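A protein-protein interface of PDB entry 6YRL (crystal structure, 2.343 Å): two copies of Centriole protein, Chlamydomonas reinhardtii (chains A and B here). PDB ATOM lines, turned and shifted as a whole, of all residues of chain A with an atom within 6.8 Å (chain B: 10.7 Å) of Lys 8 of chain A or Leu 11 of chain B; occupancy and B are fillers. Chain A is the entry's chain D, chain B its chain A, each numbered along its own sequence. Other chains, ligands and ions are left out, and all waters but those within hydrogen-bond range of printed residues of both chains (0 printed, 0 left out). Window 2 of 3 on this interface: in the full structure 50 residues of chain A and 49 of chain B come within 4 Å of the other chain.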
ATOM      1  N   ARG A   5      29.038 -22.474 -12.365  1.00  0.00           N
ATOM      2  CA  ARG A   5      29.616 -21.461 -13.240  1.00  0.00           C
ATOM      3  C   ARG A   5      30.813 -20.794 -12.567  1.00  0.00           C
ATOM      4  O   ARG A   5      31.624 -21.465 -11.929  1.00  0.00           O
ATOM      5  CB  ARG A   5      28.557 -20.424 -13.607  1.00  0.00           C
ATOM      6  CG  ARG A   5      27.698 -19.988 -12.427  1.00  0.00           C
ATOM      7  CD  ARG A   5      26.352 -19.413 -12.872  1.00  0.00           C
ATOM      8  NE  ARG A   5      26.436 -18.616 -14.095  1.00  0.00           N
ATOM      9  CZ  ARG A   5      27.159 -17.505 -14.241  1.00  0.00           C
ATOM     10  NH1 ARG A   5      27.892 -17.030 -13.239  1.00  0.00           N
ATOM     11  NH2 ARG A   5      27.155 -16.866 -15.403  1.00  0.00           N
ATOM     12  N   GLU A   6      30.929 -19.471 -12.722  1.00  0.00           N
ATOM     13  CA  GLU A   6      31.886 -18.720 -11.915  1.00  0.00           C
ATOM     14  C   GLU A   6      31.449 -18.674 -10.451  1.00  0.00           C
ATOM     15  O   GLU A   6      32.294 -18.706  -9.542  1.00  0.00           O
ATOM     16  CB  GLU A   6      32.041 -17.306 -12.480  1.00  0.00           C
ATOM     17  CG  GLU A   6      33.375 -17.027 -13.178  1.00  0.00           C
ATOM     18  CD  GLU A   6      33.376 -15.705 -13.944  1.00  0.00           C
ATOM     19  OE1 GLU A   6      32.621 -14.787 -13.552  1.00  0.00           O
ATOM     20  OE2 GLU A   6      34.130 -15.581 -14.937  1.00  0.00           O
ATOM     21  N   VAL A   7      30.134 -18.630 -10.211  1.00  0.00           N
ATOM     22  CA  VAL A   7      29.614 -18.549  -8.850  1.00  0.00           C
ATOM     23  C   VAL A   7      29.908 -19.832  -8.078  1.00  0.00           C
ATOM     24  O   VAL A   7      30.319 -19.787  -6.912  1.00  0.00           O
ATOM     25  CB  VAL A   7      28.107 -18.228  -8.883  1.00  0.00           C
ATOM     26  CG1 VAL A   7      27.405 -18.792  -7.652  1.00  0.00           C
ATOM     27  CG2 VAL A   7      27.894 -16.720  -8.983  1.00  0.00           C
ATOM     28  N   LYS A   8      29.709 -20.992  -8.709  1.00  0.00           N
ATOM     29  CA  LYS A   8      30.077 -22.250  -8.066  1.00  0.00           C
ATOM     30  C   LYS A   8      31.571 -22.302  -7.772  1.00  0.00           C
ATOM     31  O   LYS A   8      31.990 -22.901  -6.775  1.00  0.00           O
ATOM     32  CB  LYS A   8      29.658 -23.430  -8.945  1.00  0.00           C
ATOM     33  CG  LYS A   8      30.013 -24.807  -8.386  1.00  0.00           C
ATOM     34  CD  LYS A   8      31.182 -25.431  -9.135  1.00  0.00           C
ATOM     35  CE  LYS A   8      31.272 -26.926  -8.868  1.00  0.00           C
ATOM     36  NZ  LYS A   8      31.448 -27.220  -7.419  1.00  0.00           N
ATOM     37  N   TYR A   9      32.385 -21.675  -8.626  1.00  0.00           N
ATOM     38  CA  TYR A   9      33.824 -21.601  -8.391  1.00  0.00           C
ATOM     39  C   TYR A   9      34.124 -20.820  -7.113  1.00  0.00           C
ATOM     40  O   TYR A   9      34.891 -21.275  -6.248  1.00  0.00           O
ATOM     41  CB  TYR A   9      34.492 -20.965  -9.612  1.00  0.00           C
ATOM     42  CG  TYR A   9      35.998 -20.901  -9.594  1.00  0.00           C
ATOM     43  CD1 TYR A   9      36.665 -19.934  -8.850  1.00  0.00           C
ATOM     44  CD2 TYR A   9      36.756 -21.780 -10.352  1.00  0.00           C
ATOM     45  CE1 TYR A   9      38.049 -19.858  -8.843  1.00  0.00           C
ATOM     46  CE2 TYR A   9      38.140 -21.712 -10.354  1.00  0.00           C
ATOM     47  CZ  TYR A   9      38.783 -20.752  -9.596  1.00  0.00           C
ATOM     48  OH  TYR A   9      40.161 -20.684  -9.594  1.00  0.00           O
ATOM     49  N   GLU A  10      33.509 -19.641  -6.971  1.00  0.00           N
ATOM     50  CA  GLU A  10      33.645 -18.891  -5.725  1.00  0.00           C
ATOM     51  C   GLU A  10      33.182 -19.716  -4.531  1.00  0.00           C
ATOM     52  O   GLU A  10      33.889 -19.812  -3.523  1.00  0.00           O
ATOM     53  CB  GLU A  10      32.864 -17.582  -5.809  1.00  0.00           C
ATOM     54  CG  GLU A  10      33.644 -16.451  -6.471  1.00  0.00           C
ATOM     55  CD  GLU A  10      33.106 -15.069  -6.136  1.00  0.00           C
ATOM     56  OE1 GLU A  10      33.928 -14.187  -5.810  1.00  0.00           O
ATOM     57  OE2 GLU A  10      31.874 -14.858  -6.206  1.00  0.00           O
ATOM     58  N   LEU A  11      32.012 -20.344  -4.638  1.00  0.00           N
ATOM     59  CA  LEU A  11      31.494 -21.121  -3.517  1.00  0.00           C
ATOM     60  C   LEU A  11      32.454 -22.232  -3.120  1.00  0.00           C
ATOM     61  O   LEU A  11      32.683 -22.460  -1.928  1.00  0.00           O
ATOM     62  CB  LEU A  11      30.122 -21.697  -3.863  1.00  0.00           C
ATOM     63  CG  LEU A  11      28.945 -20.882  -3.331  1.00  0.00           C
ATOM     64  CD1 LEU A  11      29.172 -19.391  -3.579  1.00  0.00           C
ATOM     65  CD2 LEU A  11      27.614 -21.338  -3.936  1.00  0.00           C
ATOM     66  N   ASP A  12      33.016 -22.940  -4.097  1.00  0.00           N
ATOM     67  CA  ASP A  12      34.015 -23.955  -3.788  1.00  0.00           C
ATOM     68  C   ASP A  12      35.189 -23.353  -3.030  1.00  0.00           C
ATOM     69  O   ASP A  12      35.626 -23.907  -2.012  1.00  0.00           O
ATOM     70  CB  ASP A  12      34.481 -24.628  -5.074  1.00  0.00           C
ATOM     71  CG  ASP A  12      33.503 -25.667  -5.568  1.00  0.00           C
ATOM     72  OD1 ASP A  12      32.632 -26.089  -4.774  1.00  0.00           O
ATOM     73  OD2 ASP A  12      33.606 -26.066  -6.746  1.00  0.00           O
ATOM     74  N   THR A  13      35.697 -22.206  -3.493  1.00  0.00           N
ATOM     75  CA  THR A  13      36.792 -21.550  -2.779  1.00  0.00           C
ATOM     76  C   THR A  13      36.405 -21.229  -1.335  1.00  0.00           C
ATOM     77  O   THR A  13      37.207 -21.402  -0.405  1.00  0.00           O
ATOM     78  CB  THR A  13      37.214 -20.281  -3.518  1.00  0.00           C
ATOM     79  OG1 THR A  13      37.331 -20.556  -4.918  1.00  0.00           O
ATOM     80  CG2 THR A  13      38.544 -19.771  -2.991  1.00  0.00           C
ATOM     81  N   VAL A  15      33.982 -22.669   0.606  1.00  0.00           N
ATOM     82  CA  VAL A  15      33.886 -23.913   1.372  1.00  0.00           C
ATOM     83  C   VAL A  15      35.274 -24.419   1.739  1.00  0.00           C
ATOM     84  O   VAL A  15      35.500 -24.898   2.857  1.00  0.00           O
ATOM     85  CB  VAL A  15      33.099 -24.985   0.592  1.00  0.00           C
ATOM     86  CG1 VAL A  15      33.132 -26.327   1.338  1.00  0.00           C
ATOM     87  CG2 VAL A  15      31.673 -24.553   0.378  1.00  0.00           C
ATOM     88  N   TYR B   9      22.805 -24.226  -4.181  1.00  0.00           N
ATOM     89  CA  TYR B   9      22.081 -24.281  -2.912  1.00  0.00           C
ATOM     90  C   TYR B   9      22.802 -25.150  -1.889  1.00  0.00           C
ATOM     91  O   TYR B   9      22.949 -24.765  -0.724  1.00  0.00           O
ATOM     92  CB  TYR B   9      20.659 -24.811  -3.121  1.00  0.00           C
ATOM     93  CG  TYR B   9      19.957 -25.203  -1.834  1.00  0.00           C
ATOM     94  CD1 TYR B   9      20.011 -26.510  -1.347  1.00  0.00           C
ATOM     95  CD2 TYR B   9      19.250 -24.262  -1.097  1.00  0.00           C
ATOM     96  CE1 TYR B   9      19.376 -26.863  -0.167  1.00  0.00           C
ATOM     97  CE2 TYR B   9      18.611 -24.608   0.078  1.00  0.00           C
ATOM     98  CZ  TYR B   9      18.674 -25.907   0.541  1.00  0.00           C
ATOM     99  OH  TYR B   9      18.034 -26.238   1.715  1.00  0.00           O
ATOM    100  N   GLU B  10      23.212 -26.343  -2.333  1.00  0.00           N
ATOM    101  CA  GLU B  10      23.933 -27.265  -1.459  1.00  0.00           C
ATOM    102  C   GLU B  10      25.207 -26.625  -0.915  1.00  0.00           C
ATOM    103  O   GLU B  10      25.509 -26.729   0.285  1.00  0.00           O
ATOM    104  CB  GLU B  10      24.249 -28.551  -2.227  1.00  0.00           C
ATOM    105  CG  GLU B  10      24.941 -29.633  -1.414  1.00  0.00           C
ATOM    106  CD  GLU B  10      24.307 -29.835  -0.053  1.00  0.00           C
ATOM    107  OE1 GLU B  10      24.929 -29.442   0.960  1.00  0.00           O
ATOM    108  OE2 GLU B  10      23.184 -30.382   0.000  1.00  0.00           O
ATOM    109  N   LEU B  11      25.960 -25.945  -1.783  1.00  0.00           N
ATOM    110  CA  LEU B  11      27.159 -25.252  -1.328  1.00  0.00           C
ATOM    111  C   LEU B  11      26.818 -24.175  -0.303  1.00  0.00           C
ATOM    112  O   LEU B  11      27.569 -23.967   0.654  1.00  0.00           O
ATOM    113  CB  LEU B  11      27.910 -24.659  -2.521  1.00  0.00           C
ATOM    114  CG  LEU B  11      28.622 -25.683  -3.411  1.00  0.00           C
ATOM    115  CD1 LEU B  11      29.164 -25.024  -4.666  1.00  0.00           C
ATOM    116  CD2 LEU B  11      29.738 -26.386  -2.647  1.00  0.00           C
ATOM    117  N   ASP B  12      25.679 -23.492  -0.473  1.00  0.00           N
ATOM    118  CA  ASP B  12      25.262 -22.493   0.511  1.00  0.00           C
ATOM    119  C   ASP B  12      25.042 -23.127   1.884  1.00  0.00           C
ATOM    120  O   ASP B  12      25.474 -22.582   2.912  1.00  0.00           O
ATOM    121  CB  ASP B  12      23.987 -21.786   0.032  1.00  0.00           C
ATOM    122  CG  ASP B  12      24.269 -20.649  -0.951  1.00  0.00           C
ATOM    123  OD1 ASP B  12      25.373 -20.612  -1.538  1.00  0.00           O
ATOM    124  OD2 ASP B  12      23.374 -19.791  -1.138  1.00  0.00           O
ATOM    125  N   THR B  13      24.376 -24.286   1.916  1.00  0.00           N
ATOM    126  CA  THR B  13      24.162 -25.006   3.168  1.00  0.00           C
ATOM    127  C   THR B  13      25.485 -25.385   3.820  1.00  0.00           C
ATOM    128  O   THR B  13      25.665 -25.214   5.034  1.00  0.00           O
ATOM    129  CB  THR B  13      23.324 -26.262   2.920  1.00  0.00           C
ATOM    130  OG1 THR B  13      22.028 -25.890   2.438  1.00  0.00           O
ATOM    131  CG2 THR B  13      23.177 -27.070   4.205  1.00  0.00           C
ATOM    132  N   LYS B  14      26.427 -25.915   3.028  1.00  0.00           N
ATOM    133  CA  LYS B  14      27.705 -26.325   3.610  1.00  0.00           C
ATOM    134  C   LYS B  14      28.504 -25.121   4.107  1.00  0.00           C
ATOM    135  O   LYS B  14      29.137 -25.186   5.168  1.00  0.00           O
ATOM    136  CB  LYS B  14      28.514 -27.146   2.603  1.00  0.00           C
ATOM    137  CG  LYS B  14      29.750 -27.801   3.211  1.00  0.00           C
ATOM    138  CD  LYS B  14      29.762 -29.321   3.022  1.00  0.00           C
ATOM    139  CE  LYS B  14      30.375 -29.738   1.683  1.00  0.00           C
ATOM    140  NZ  LYS B  14      30.182 -31.187   1.374  1.00  0.00           N
ATOM    141  N   VAL B  15      28.474 -24.011   3.365  1.00  0.00           N
ATOM    142  CA  VAL B  15      29.073 -22.773   3.859  1.00  0.00           C
ATOM    143  C   VAL B  15      28.457 -22.388   5.197  1.00  0.00           C
ATOM    144  O   VAL B  15      29.151 -21.926   6.111  1.00  0.00           O
ATOM    145  CB  VAL B  15      28.917 -21.644   2.822  1.00  0.00           C
ATOM    146  CG1 VAL B  15      29.293 -20.300   3.432  1.00  0.00           C
ATOM    147  CG2 VAL B  15      29.768 -21.914   1.604  1.00  0.00           C
ATOM    148  N   SER B  16      27.147 -22.595   5.345  1.00  0.00           N
ATOM    149  CA  SER B  16      26.476 -22.176   6.573  1.00  0.00           C
ATOM    150  C   SER B  16      26.889 -23.041   7.761  1.00  0.00           C
ATOM    151  O   SER B  16      27.374 -22.527   8.780  1.00  0.00           O
ATOM    152  CB  SER B  16      24.963 -22.198   6.369  1.00  0.00           C
ATOM    153  OG  SER B  16      24.513 -20.916   5.970  1.00  0.00           O
ATOM    154  N   GLU B  17      26.705 -24.363   7.657  1.00  0.00           N
ATOM    155  CA  GLU B  17      27.126 -25.240   8.747  1.00  0.00           C
ATOM    156  C   GLU B  17      28.614 -25.068   9.068  1.00  0.00           C
ATOM    157  O   GLU B  17      29.010 -25.146  10.241  1.00  0.00           O
ATOM    158  CB  GLU B  17      26.785 -26.697   8.408  1.00  0.00           C
ATOM    159  CG  GLU B  17      27.875 -27.485   7.683  1.00  0.00           C
ATOM    160  CD  GLU B  17      27.403 -28.856   7.222  1.00  0.00           C
ATOM    161  OE1 GLU B  17      26.199 -28.997   6.914  1.00  0.00           O
ATOM    162  OE2 GLU B  17      28.236 -29.789   7.169  1.00  0.00           O
ATOM    163  N   LEU B  18      29.445 -24.790   8.055  1.00  0.00           N
ATOM    164  CA  LEU B  18      30.867 -24.565   8.306  1.00  0.00           C
ATOM    165  C   LEU B  18      31.093 -23.275   9.088  1.00  0.00           C
ATOM    166  O   LEU B  18      31.864 -23.250  10.054  1.00  0.00           O
ATOM    167  CB  LEU B  18      31.644 -24.541   6.987  1.00  0.00           C
ATOM    168  CG  LEU B  18      32.013 -25.905   6.399  1.00  0.00           C
ATOM    169  CD1 LEU B  18      32.997 -25.745   5.253  1.00  0.00           C
ATOM    170  CD2 LEU B  18      32.579 -26.831   7.470  1.00  0.00           C
ATOM    171  N   SER B  19      30.427 -22.190   8.690  1.00  0.00           N
ATOM    172  CA  SER B  19      30.589 -20.930   9.409  1.00  0.00           C
ATOM    173  C   SER B  19      30.121 -21.061  10.853  1.00  0.00           C
ATOM    174  O   SER B  19      30.713 -20.468  11.767  1.00  0.00           O
ATOM    175  CB  SER B  19      29.821 -19.819   8.696  1.00  0.00           C
ATOM    176  OG  SER B  19      29.924 -19.942   7.285  1.00  0.00           O
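The backbone carbonyl oxygen of Val 15 of chain B lies within hydrogen-bond range of the side-chain hydroxyl of Ser 19 of chain B (2.4 Å).
NZ of Lys 8 of chain A is in salt-bridge range of OD2 of Asp 12 of chain A, 2.5 Å away.
Printed residues of chain A that touch a printed residue of chain B: Lys 8, Leu 11, Asp 12 and Val 15.
Hydrophobic or aromatic side chains of chain A within 4 Å of the printed part of chain B: Leu 11 and Val 15.
Of the 11 printed residues of chain B, 4 touch a printed residue of chain A.
Printed residues of chain B that touch a printed residue of chain A: Leu 11, Asp 12, Val 15 and Leu 18.
Hydrophobic or aromatic side chains of chain B within 4 Å of the printed part of chain A: Leu 11, Val 15 and Leu 18.
Leu 11 of chain A touches its own counterpart, Leu 11 of chain B.
Leu 11 of chain A touches Asp 12 of chain B, and with the chains exchanged Asp 12 of chain A touches Leu 11 of chain B.
Val 15 of chain A touches its own counterpart, Val 15 of chain B.
Positions printed for both chains: 9, 10, 11, 12, 13 and 15.
Of the 6 pairs that touch across the chains among the printed residues, 4 have their exchanged pair printed and touching as well.
Among the printed residues, merely in contact across the chains: Leu 11 of chain A with Asp 12 of chain B, Val 15 of chain A with Val 15 of chain B, Leu 11 of chain A with Leu 11 of chain B, Val 15 of chain A with Leu 18 of chain B, Asp 12 of chain A with Leu 11 of chain B and Lys 8 of chain A with Leu 11 of chain B.
No residue of chain B comes within 4 Å of Val 7 of chain A.
Of chain B, only Leu 11 (3.6 Å) and Asp 12 (3.4 Å) come within 4 Å of Leu 11 of chain A.
Asp 12 of chain A touches just one residue of chain B: Leu 11 (3.6 Å).
Of the printed residues of chain B, Val 15 of chain A touches Val 15 and Leu 18.
Leu 11 of chain B touches just these residues of chain A: Lys 8, Leu 11 and Asp 12.
Of the printed residues of chain A, Asp 12 of chain B touches Leu 11 (3.4 Å).
Lys 14 of chain B touches none of the printed residues of chain A.
Printed residues of chain A within 4 Å of Leu 18 of chain B: Val 15 (3.6 Å).
The nearest residue of chain B that does not touch Lys 8 of chain A is Asp 12 of chain B (8.2 Å).
The nearest residue of chain A that does not touch Leu 11 of chain B is Val 15 of chain A (4.03 Å).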
